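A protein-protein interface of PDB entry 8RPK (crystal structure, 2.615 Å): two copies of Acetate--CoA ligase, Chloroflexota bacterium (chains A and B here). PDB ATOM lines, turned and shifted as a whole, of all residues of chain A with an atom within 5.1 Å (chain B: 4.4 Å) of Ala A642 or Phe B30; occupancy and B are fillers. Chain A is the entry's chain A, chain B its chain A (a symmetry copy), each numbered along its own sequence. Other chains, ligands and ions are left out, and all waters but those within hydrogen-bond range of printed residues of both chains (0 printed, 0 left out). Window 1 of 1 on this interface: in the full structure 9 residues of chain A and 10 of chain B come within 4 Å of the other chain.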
ATOM      1  N   ARG A 638      23.133  -6.180  -7.187  1.00  0.00           N
ATOM      2  CA  ARG A 638      22.416  -6.468  -5.953  1.00  0.00           C
ATOM      3  C   ARG A 638      23.379  -7.051  -4.920  1.00  0.00           C
ATOM      4  O   ARG A 638      23.281  -6.702  -3.740  1.00  0.00           O
ATOM      5  CB  ARG A 638      21.223  -7.408  -6.174  1.00  0.00           C
ATOM      6  CG  ARG A 638      20.281  -6.903  -7.253  1.00  0.00           C
ATOM      7  CD  ARG A 638      18.841  -6.960  -6.780  1.00  0.00           C
ATOM      8  NE  ARG A 638      17.909  -6.595  -7.855  1.00  0.00           N
ATOM      9  CZ  ARG A 638      17.012  -7.409  -8.428  1.00  0.00           C
ATOM     10  NH1 ARG A 638      16.816  -8.645  -7.988  1.00  0.00           N
ATOM     11  NH2 ARG A 638      16.285  -6.978  -9.445  1.00  0.00           N
ATOM     12  N   VAL A 639      24.283  -7.933  -5.381  1.00  0.00           N
ATOM     13  CA  VAL A 639      25.268  -8.590  -4.532  1.00  0.00           C
ATOM     14  C   VAL A 639      26.206  -7.533  -3.948  1.00  0.00           C
ATOM     15  O   VAL A 639      26.500  -7.572  -2.754  1.00  0.00           O
ATOM     16  CB  VAL A 639      26.069  -9.674  -5.287  1.00  0.00           C
ATOM     17  CG1 VAL A 639      27.124 -10.336  -4.417  1.00  0.00           C
ATOM     18  CG2 VAL A 639      25.167 -10.766  -5.834  1.00  0.00           C
ATOM     19  N   VAL A 640      26.643  -6.594  -4.799  1.00  0.00           N
ATOM     20  CA  VAL A 640      27.555  -5.528  -4.424  1.00  0.00           C
ATOM     21  C   VAL A 640      26.960  -4.753  -3.253  1.00  0.00           C
ATOM     22  O   VAL A 640      27.644  -4.520  -2.242  1.00  0.00           O
ATOM     23  CB  VAL A 640      27.830  -4.594  -5.625  1.00  0.00           C
ATOM     24  CG1 VAL A 640      28.575  -3.316  -5.226  1.00  0.00           C
ATOM     25  CG2 VAL A 640      28.568  -5.301  -6.765  1.00  0.00           C
ATOM     26  N   ARG A 641      25.683  -4.365  -3.407  1.00  0.00           N
ATOM     27  CA  ARG A 641      24.988  -3.581  -2.392  1.00  0.00           C
ATOM     28  C   ARG A 641      24.809  -4.406  -1.123  1.00  0.00           C
ATOM     29  O   ARG A 641      24.921  -3.876  -0.029  1.00  0.00           O
ATOM     30  CB  ARG A 641      23.619  -3.143  -2.897  1.00  0.00           C
ATOM     31  CG  ARG A 641      22.914  -2.090  -2.058  1.00  0.00           C
ATOM     32  CD  ARG A 641      21.635  -1.569  -2.753  1.00  0.00           C
ATOM     33  NE  ARG A 641      21.174  -0.372  -2.037  1.00  0.00           N
ATOM     34  CZ  ARG A 641      20.627  -0.337  -0.819  1.00  0.00           C
ATOM     35  NH1 ARG A 641      20.085  -1.420  -0.297  1.00  0.00           N
ATOM     36  NH2 ARG A 641      20.568   0.803  -0.145  1.00  0.00           N
ATOM     37  N   ALA A 642      24.550  -5.705  -1.290  1.00  0.00           N
ATOM     38  CA  ALA A 642      24.271  -6.597  -0.181  1.00  0.00           C
ATOM     39  C   ALA A 642      25.547  -6.892   0.597  1.00  0.00           C
ATOM     40  O   ALA A 642      25.460  -7.211   1.788  1.00  0.00           O
ATOM     41  CB  ALA A 642      23.622  -7.883  -0.689  1.00  0.00           C
ATOM     42  N   ARG A 643      26.706  -6.845  -0.086  1.00  0.00           N
ATOM     43  CA  ARG A 643      27.992  -6.965   0.588  1.00  0.00           C
ATOM     44  C   ARG A 643      28.176  -5.756   1.504  1.00  0.00           C
ATOM     45  O   ARG A 643      28.579  -5.917   2.658  1.00  0.00           O
ATOM     46  CB  ARG A 643      29.180  -7.137  -0.368  1.00  0.00           C
ATOM     47  CG  ARG A 643      29.263  -8.534  -0.966  1.00  0.00           C
ATOM     48  CD  ARG A 643      30.559  -8.839  -1.727  1.00  0.00           C
ATOM     49  NE  ARG A 643      30.566 -10.145  -2.417  1.00  0.00           N
ATOM     50  CZ  ARG A 643      31.011 -10.403  -3.663  1.00  0.00           C
ATOM     51  NH1 ARG A 643      31.463  -9.417  -4.417  1.00  0.00           N
ATOM     52  NH2 ARG A 643      31.017 -11.632  -4.173  1.00  0.00           N
ATOM     53  N   GLU A 644      27.828  -4.561   1.004  1.00  0.00           N
ATOM     54  CA  GLU A 644      27.983  -3.341   1.781  1.00  0.00           C
ATOM     55  C   GLU A 644      26.927  -3.228   2.870  1.00  0.00           C
ATOM     56  O   GLU A 644      27.292  -2.897   3.977  1.00  0.00           O
ATOM     57  CB  GLU A 644      27.857  -2.031   1.002  1.00  0.00           C
ATOM     58  CG  GLU A 644      29.158  -1.563   0.349  1.00  0.00           C
ATOM     59  CD  GLU A 644      29.952  -0.487   1.077  1.00  0.00           C
ATOM     60  OE1 GLU A 644      29.566   0.700   1.138  1.00  0.00           O
ATOM     61  OE2 GLU A 644      31.005  -0.873   1.598  1.00  0.00           O
ATOM     62  N   LEU A 645      25.642  -3.433   2.545  1.00  0.00           N
ATOM     63  CA  LEU A 645      24.527  -2.997   3.382  1.00  0.00           C
ATOM     64  C   LEU A 645      23.641  -4.156   3.807  1.00  0.00           C
ATOM     65  O   LEU A 645      22.686  -3.913   4.536  1.00  0.00           O
ATOM     66  CB  LEU A 645      23.646  -1.979   2.655  1.00  0.00           C
ATOM     67  CG  LEU A 645      24.297  -0.653   2.245  1.00  0.00           C
ATOM     68  CD1 LEU A 645      23.279   0.230   1.554  1.00  0.00           C
ATOM     69  CD2 LEU A 645      24.912   0.088   3.426  1.00  0.00           C
ATOM     70  N   GLY A 646      23.897  -5.371   3.294  1.00  0.00           N
ATOM     71  CA  GLY A 646      23.025  -6.517   3.524  1.00  0.00           C
ATOM     72  C   GLY A 646      21.725  -6.425   2.723  1.00  0.00           C
ATOM     73  O   GLY A 646      21.267  -5.331   2.391  1.00  0.00           O
ATOM     74  N   GLU A 647      21.127  -7.591   2.425  1.00  0.00           N
ATOM     75  CA  GLU A 647      19.840  -7.654   1.747  1.00  0.00           C
ATOM     76  C   GLU A 647      18.808  -8.092   2.772  1.00  0.00           C
ATOM     77  O   GLU A 647      19.079  -9.037   3.516  1.00  0.00           O
ATOM     78  CB  GLU A 647      19.866  -8.624   0.567  1.00  0.00           C
ATOM     79  CG  GLU A 647      18.979  -8.182  -0.599  1.00  0.00           C
ATOM     80  CD  GLU A 647      19.639  -8.419  -1.956  1.00  0.00           C
ATOM     81  OE1 GLU A 647      20.266  -9.504  -2.089  1.00  0.00           O
ATOM     82  OE2 GLU A 647      19.558  -7.553  -2.869  1.00  0.00           O
ATOM     83  N   ARG B  28      18.964  -9.057   8.136  1.00  0.00           N
ATOM     84  CA  ARG B  28      19.580  -8.745   6.858  1.00  0.00           C
ATOM     85  C   ARG B  28      20.637  -9.780   6.534  1.00  0.00           C
ATOM     86  O   ARG B  28      21.381 -10.211   7.410  1.00  0.00           O
ATOM     87  CB  ARG B  28      20.225  -7.365   6.905  1.00  0.00           C
ATOM     88  CG  ARG B  28      19.241  -6.281   7.305  1.00  0.00           C
ATOM     89  CD  ARG B  28      19.847  -4.896   7.235  1.00  0.00           C
ATOM     90  NE  ARG B  28      19.910  -4.470   5.834  1.00  0.00           N
ATOM     91  CZ  ARG B  28      19.400  -3.339   5.395  1.00  0.00           C
ATOM     92  NH1 ARG B  28      18.965  -2.437   6.268  1.00  0.00           N
ATOM     93  NH2 ARG B  28      19.353  -3.130   4.094  1.00  0.00           N
ATOM     94  N   LEU B  29      20.726 -10.134   5.255  1.00  0.00           N
ATOM     95  CA  LEU B  29      21.574 -11.234   4.843  1.00  0.00           C
ATOM     96  C   LEU B  29      22.826 -10.674   4.185  1.00  0.00           C
ATOM     97  O   LEU B  29      22.723  -9.844   3.291  1.00  0.00           O
ATOM     98  CB  LEU B  29      20.735 -12.080   3.890  1.00  0.00           C
ATOM     99  CG  LEU B  29      21.133 -13.553   3.795  1.00  0.00           C
ATOM    100  CD1 LEU B  29      20.772 -14.219   5.113  1.00  0.00           C
ATOM    101  CD2 LEU B  29      20.513 -14.304   2.608  1.00  0.00           C
ATOM    102  N   PHE B  30      24.006 -11.122   4.623  1.00  0.00           N
ATOM    103  CA  PHE B  30      25.248 -10.628   4.047  1.00  0.00           C
ATOM    104  C   PHE B  30      25.939 -11.753   3.307  1.00  0.00           C
ATOM    105  O   PHE B  30      26.355 -12.699   3.944  1.00  0.00           O
ATOM    106  CB  PHE B  30      26.221 -10.086   5.102  1.00  0.00           C
ATOM    107  CG  PHE B  30      25.728  -8.790   5.717  1.00  0.00           C
ATOM    108  CD1 PHE B  30      24.824  -8.806   6.771  1.00  0.00           C
ATOM    109  CD2 PHE B  30      26.117  -7.569   5.193  1.00  0.00           C
ATOM    110  CE1 PHE B  30      24.369  -7.624   7.328  1.00  0.00           C
ATOM    111  CE2 PHE B  30      25.648  -6.386   5.745  1.00  0.00           C
ATOM    112  CZ  PHE B  30      24.777  -6.415   6.811  1.00  0.00           C
ATOM    113  N   PRO B  31      26.097 -11.680   1.968  1.00  0.00           N
ATOM    114  CA  PRO B  31      26.572 -12.817   1.189  1.00  0.00           C
ATOM    115  C   PRO B  31      28.084 -12.872   1.298  1.00  0.00           C
ATOM    116  O   PRO B  31      28.711 -11.868   1.607  1.00  0.00           O
ATOM    117  CB  PRO B  31      26.059 -12.515  -0.217  1.00  0.00           C
ATOM    118  CG  PRO B  31      26.079 -11.005  -0.301  1.00  0.00           C
ATOM    119  CD  PRO B  31      25.806 -10.514   1.119  1.00  0.00           C
ATOM    120  N   PRO B  32      28.693 -14.067   1.149  1.00  0.00           N
ATOM    121  CA  PRO B  32      30.143 -14.213   1.261  1.00  0.00           C
ATOM    122  C   PRO B  32      30.902 -13.705   0.042  1.00  0.00           C
ATOM    123  O   PRO B  32      30.339 -13.700  -1.057  1.00  0.00           O
ATOM    124  CB  PRO B  32      30.307 -15.730   1.433  1.00  0.00           C
ATOM    125  CG  PRO B  32      29.143 -16.320   0.712  1.00  0.00           C
ATOM    126  CD  PRO B  32      28.008 -15.352   0.962  1.00  0.00           C
ATOM    127  N   TRP B 422      28.792  -6.324  16.012  1.00  0.00           N
ATOM    128  CA  TRP B 422      28.946  -7.059  14.765  1.00  0.00           C
ATOM    129  C   TRP B 422      29.256  -6.080  13.635  1.00  0.00           C
ATOM    130  O   TRP B 422      30.261  -6.245  12.949  1.00  0.00           O
ATOM    131  CB  TRP B 422      27.657  -7.855  14.493  1.00  0.00           C
ATOM    132  CG  TRP B 422      27.732  -8.896  13.412  1.00  0.00           C
ATOM    133  CD1 TRP B 422      27.917 -10.240  13.558  1.00  0.00           C
ATOM    134  CD2 TRP B 422      27.578  -8.661  12.003  1.00  0.00           C
ATOM    135  NE1 TRP B 422      27.892 -10.855  12.337  1.00  0.00           N
ATOM    136  CE2 TRP B 422      27.685  -9.914  11.369  1.00  0.00           C
ATOM    137  CE3 TRP B 422      27.370  -7.518  11.227  1.00  0.00           C
ATOM    138  CZ2 TRP B 422      27.605 -10.051   9.992  1.00  0.00           C
ATOM    139  CZ3 TRP B 422      27.267  -7.656   9.856  1.00  0.00           C
ATOM    140  CH2 TRP B 422      27.392  -8.907   9.253  1.00  0.00           C
ATOM    141  N   ARG B 426      32.769  -5.881  11.599  1.00  0.00           N
ATOM    142  CA  ARG B 426      32.825  -6.020  10.157  1.00  0.00           C
ATOM    143  C   ARG B 426      33.336  -4.744   9.478  1.00  0.00           C
ATOM    144  O   ARG B 426      34.001  -4.817   8.436  1.00  0.00           O
ATOM    145  CB  ARG B 426      31.428  -6.380   9.643  1.00  0.00           C
ATOM    146  CG  ARG B 426      31.348  -6.763   8.171  1.00  0.00           C
ATOM    147  CD  ARG B 426      29.907  -6.781   7.700  1.00  0.00           C
ATOM    148  NE  ARG B 426      29.744  -6.804   6.242  1.00  0.00           N
ATOM    149  CZ  ARG B 426      30.013  -7.849   5.442  1.00  0.00           C
ATOM    150  NH1 ARG B 426      30.531  -8.995   5.892  1.00  0.00           N
ATOM    151  NH2 ARG B 426      29.736  -7.717   4.163  1.00  0.00           N
ATOM    152  N   PRO B 457      25.685 -17.154   3.761  1.00  0.00           N
ATOM    153  CA  PRO B 457      25.228 -15.802   4.054  1.00  0.00           C
ATOM    154  C   PRO B 457      25.037 -15.637   5.560  1.00  0.00           C
ATOM    155  O   PRO B 457      24.495 -16.524   6.203  1.00  0.00           O
ATOM    156  CB  PRO B 457      23.895 -15.693   3.270  1.00  0.00           C
ATOM    157  CG  PRO B 457      23.573 -17.099   2.795  1.00  0.00           C
ATOM    158  CD  PRO B 457      24.905 -17.798   2.694  1.00  0.00           C
ATOM    159  N   LEU B 458      25.467 -14.487   6.090  1.00  0.00           N
ATOM    160  CA  LEU B 458      25.474 -14.221   7.521  1.00  0.00           C
ATOM    161  C   LEU B 458      24.338 -13.271   7.862  1.00  0.00           C
ATOM    162  O   LEU B 458      23.941 -12.433   7.048  1.00  0.00           O
ATOM    163  CB  LEU B 458      26.792 -13.591   7.953  1.00  0.00           C
ATOM    164  CG  LEU B 458      28.045 -14.224   7.351  1.00  0.00           C
ATOM    165  CD1 LEU B 458      29.179 -13.260   7.462  1.00  0.00           C
ATOM    166  CD2 LEU B 458      28.390 -15.515   8.047  1.00  0.00           C
ATOM    167  N   PRO B 460      23.500 -10.686  11.327  1.00  0.00           N
ATOM    168  CA  PRO B 460      24.121 -10.193  12.556  1.00  0.00           C
ATOM    169  C   PRO B 460      23.488 -10.774  13.815  1.00  0.00           C
ATOM    170  O   PRO B 460      22.282 -10.730  13.950  1.00  0.00           O
ATOM    171  CB  PRO B 460      23.884  -8.663  12.449  1.00  0.00           C
ATOM    172  CG  PRO B 460      23.684  -8.385  10.974  1.00  0.00           C
ATOM    173  CD  PRO B 460      22.910  -9.605  10.516  1.00  0.00           C
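The backbone carbonyl oxygen (O) of Glu A647 is in hydrogen-bond range of the backbone NH (N) of Leu B29, 2.6 Å away.
O of Gly A646 sits at hydrogen-bond distance from NH2 of Arg B28 (3.4 Å).
The guanidinium group (NE) of Arg B28 is in hydrogen-bond range of the backbone carbonyl oxygen (O) of Leu A645 (3.1 Å).
The backbone carbonyl oxygen (O) of Arg A643 lies within hydrogen-bond range of the guanidinium group (NH2) of Arg B426, at 2.6 Å.
The backbone carbonyl oxygen (O) of Leu B458 lies within hydrogen-bond range of the backbone NH (N) of Phe B30 (2.8 Å).
Among the printed residues, pairs that only touch across the chains: Gly A646 with Phe B30, Gly A646 with Leu B29, Ala A642 with Pro B31, Glu A647 with Arg B28, Ala A642 with Phe B30, Leu A645 with Phe B30, Arg A643 with Pro B32, Arg A643 with Phe B30 and Arg A643 with Pro B31.
Of chain B, only Phe B30 (3.5 Å) and Pro B31 (3.4 Å) come within 4 Å of Ala A642.
Of the printed residues of chain B, Arg A643 touches Phe B30, Pro B31, Pro B32 and Arg B426.
Printed residues of chain B within 4 Å of Gly A646: Arg B28, Leu B29 and Phe B30.
Of the printed residues of chain A, Leu B29 touches Gly A646 (3.3 Å) and Glu A647 (2.6 Å).
Printed residues of chain A within 4 Å of Pro B32: Arg A643.
Trp B422 touches none of the printed residues of chain A.
Of the printed residues of chain A, Arg B426 touches Arg A643 (2.6 Å).
Pro B460 touches none of the printed residues of chain A.
The nearest residue of chain B that does not touch Ala A642 is Leu B29 (4.1 Å).
The nearest residue of chain A that does not touch Phe B30 is Glu A644 (4.2 Å).
Of the 10 printed residues of chain B, 6 touch a printed residue of chain A.
Hydrophobic or aromatic side chains of chain B within 4 Å of the printed part of chain A: Leu B29, Phe B30 and Pro B31.
Printed residues of chain A that touch a printed residue of chain B: Ala A642, Arg A643, Leu A645, Gly A646 and Glu A647.
Hydrophobic or aromatic side chains of chain A within 4 Å of the printed part of chain B: Ala A642.
Among the printed residues, 13 pairs touch across the chains.
Among the printed residues, no Asp or Glu carboxylate lies within 4 Å of a Lys or Arg side-chain nitrogen of the other chain.
No position is printed for both chains.
Of the 13 pairs that touch across the chains among the printed residues, none has its exchanged pair printed and touching as well.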
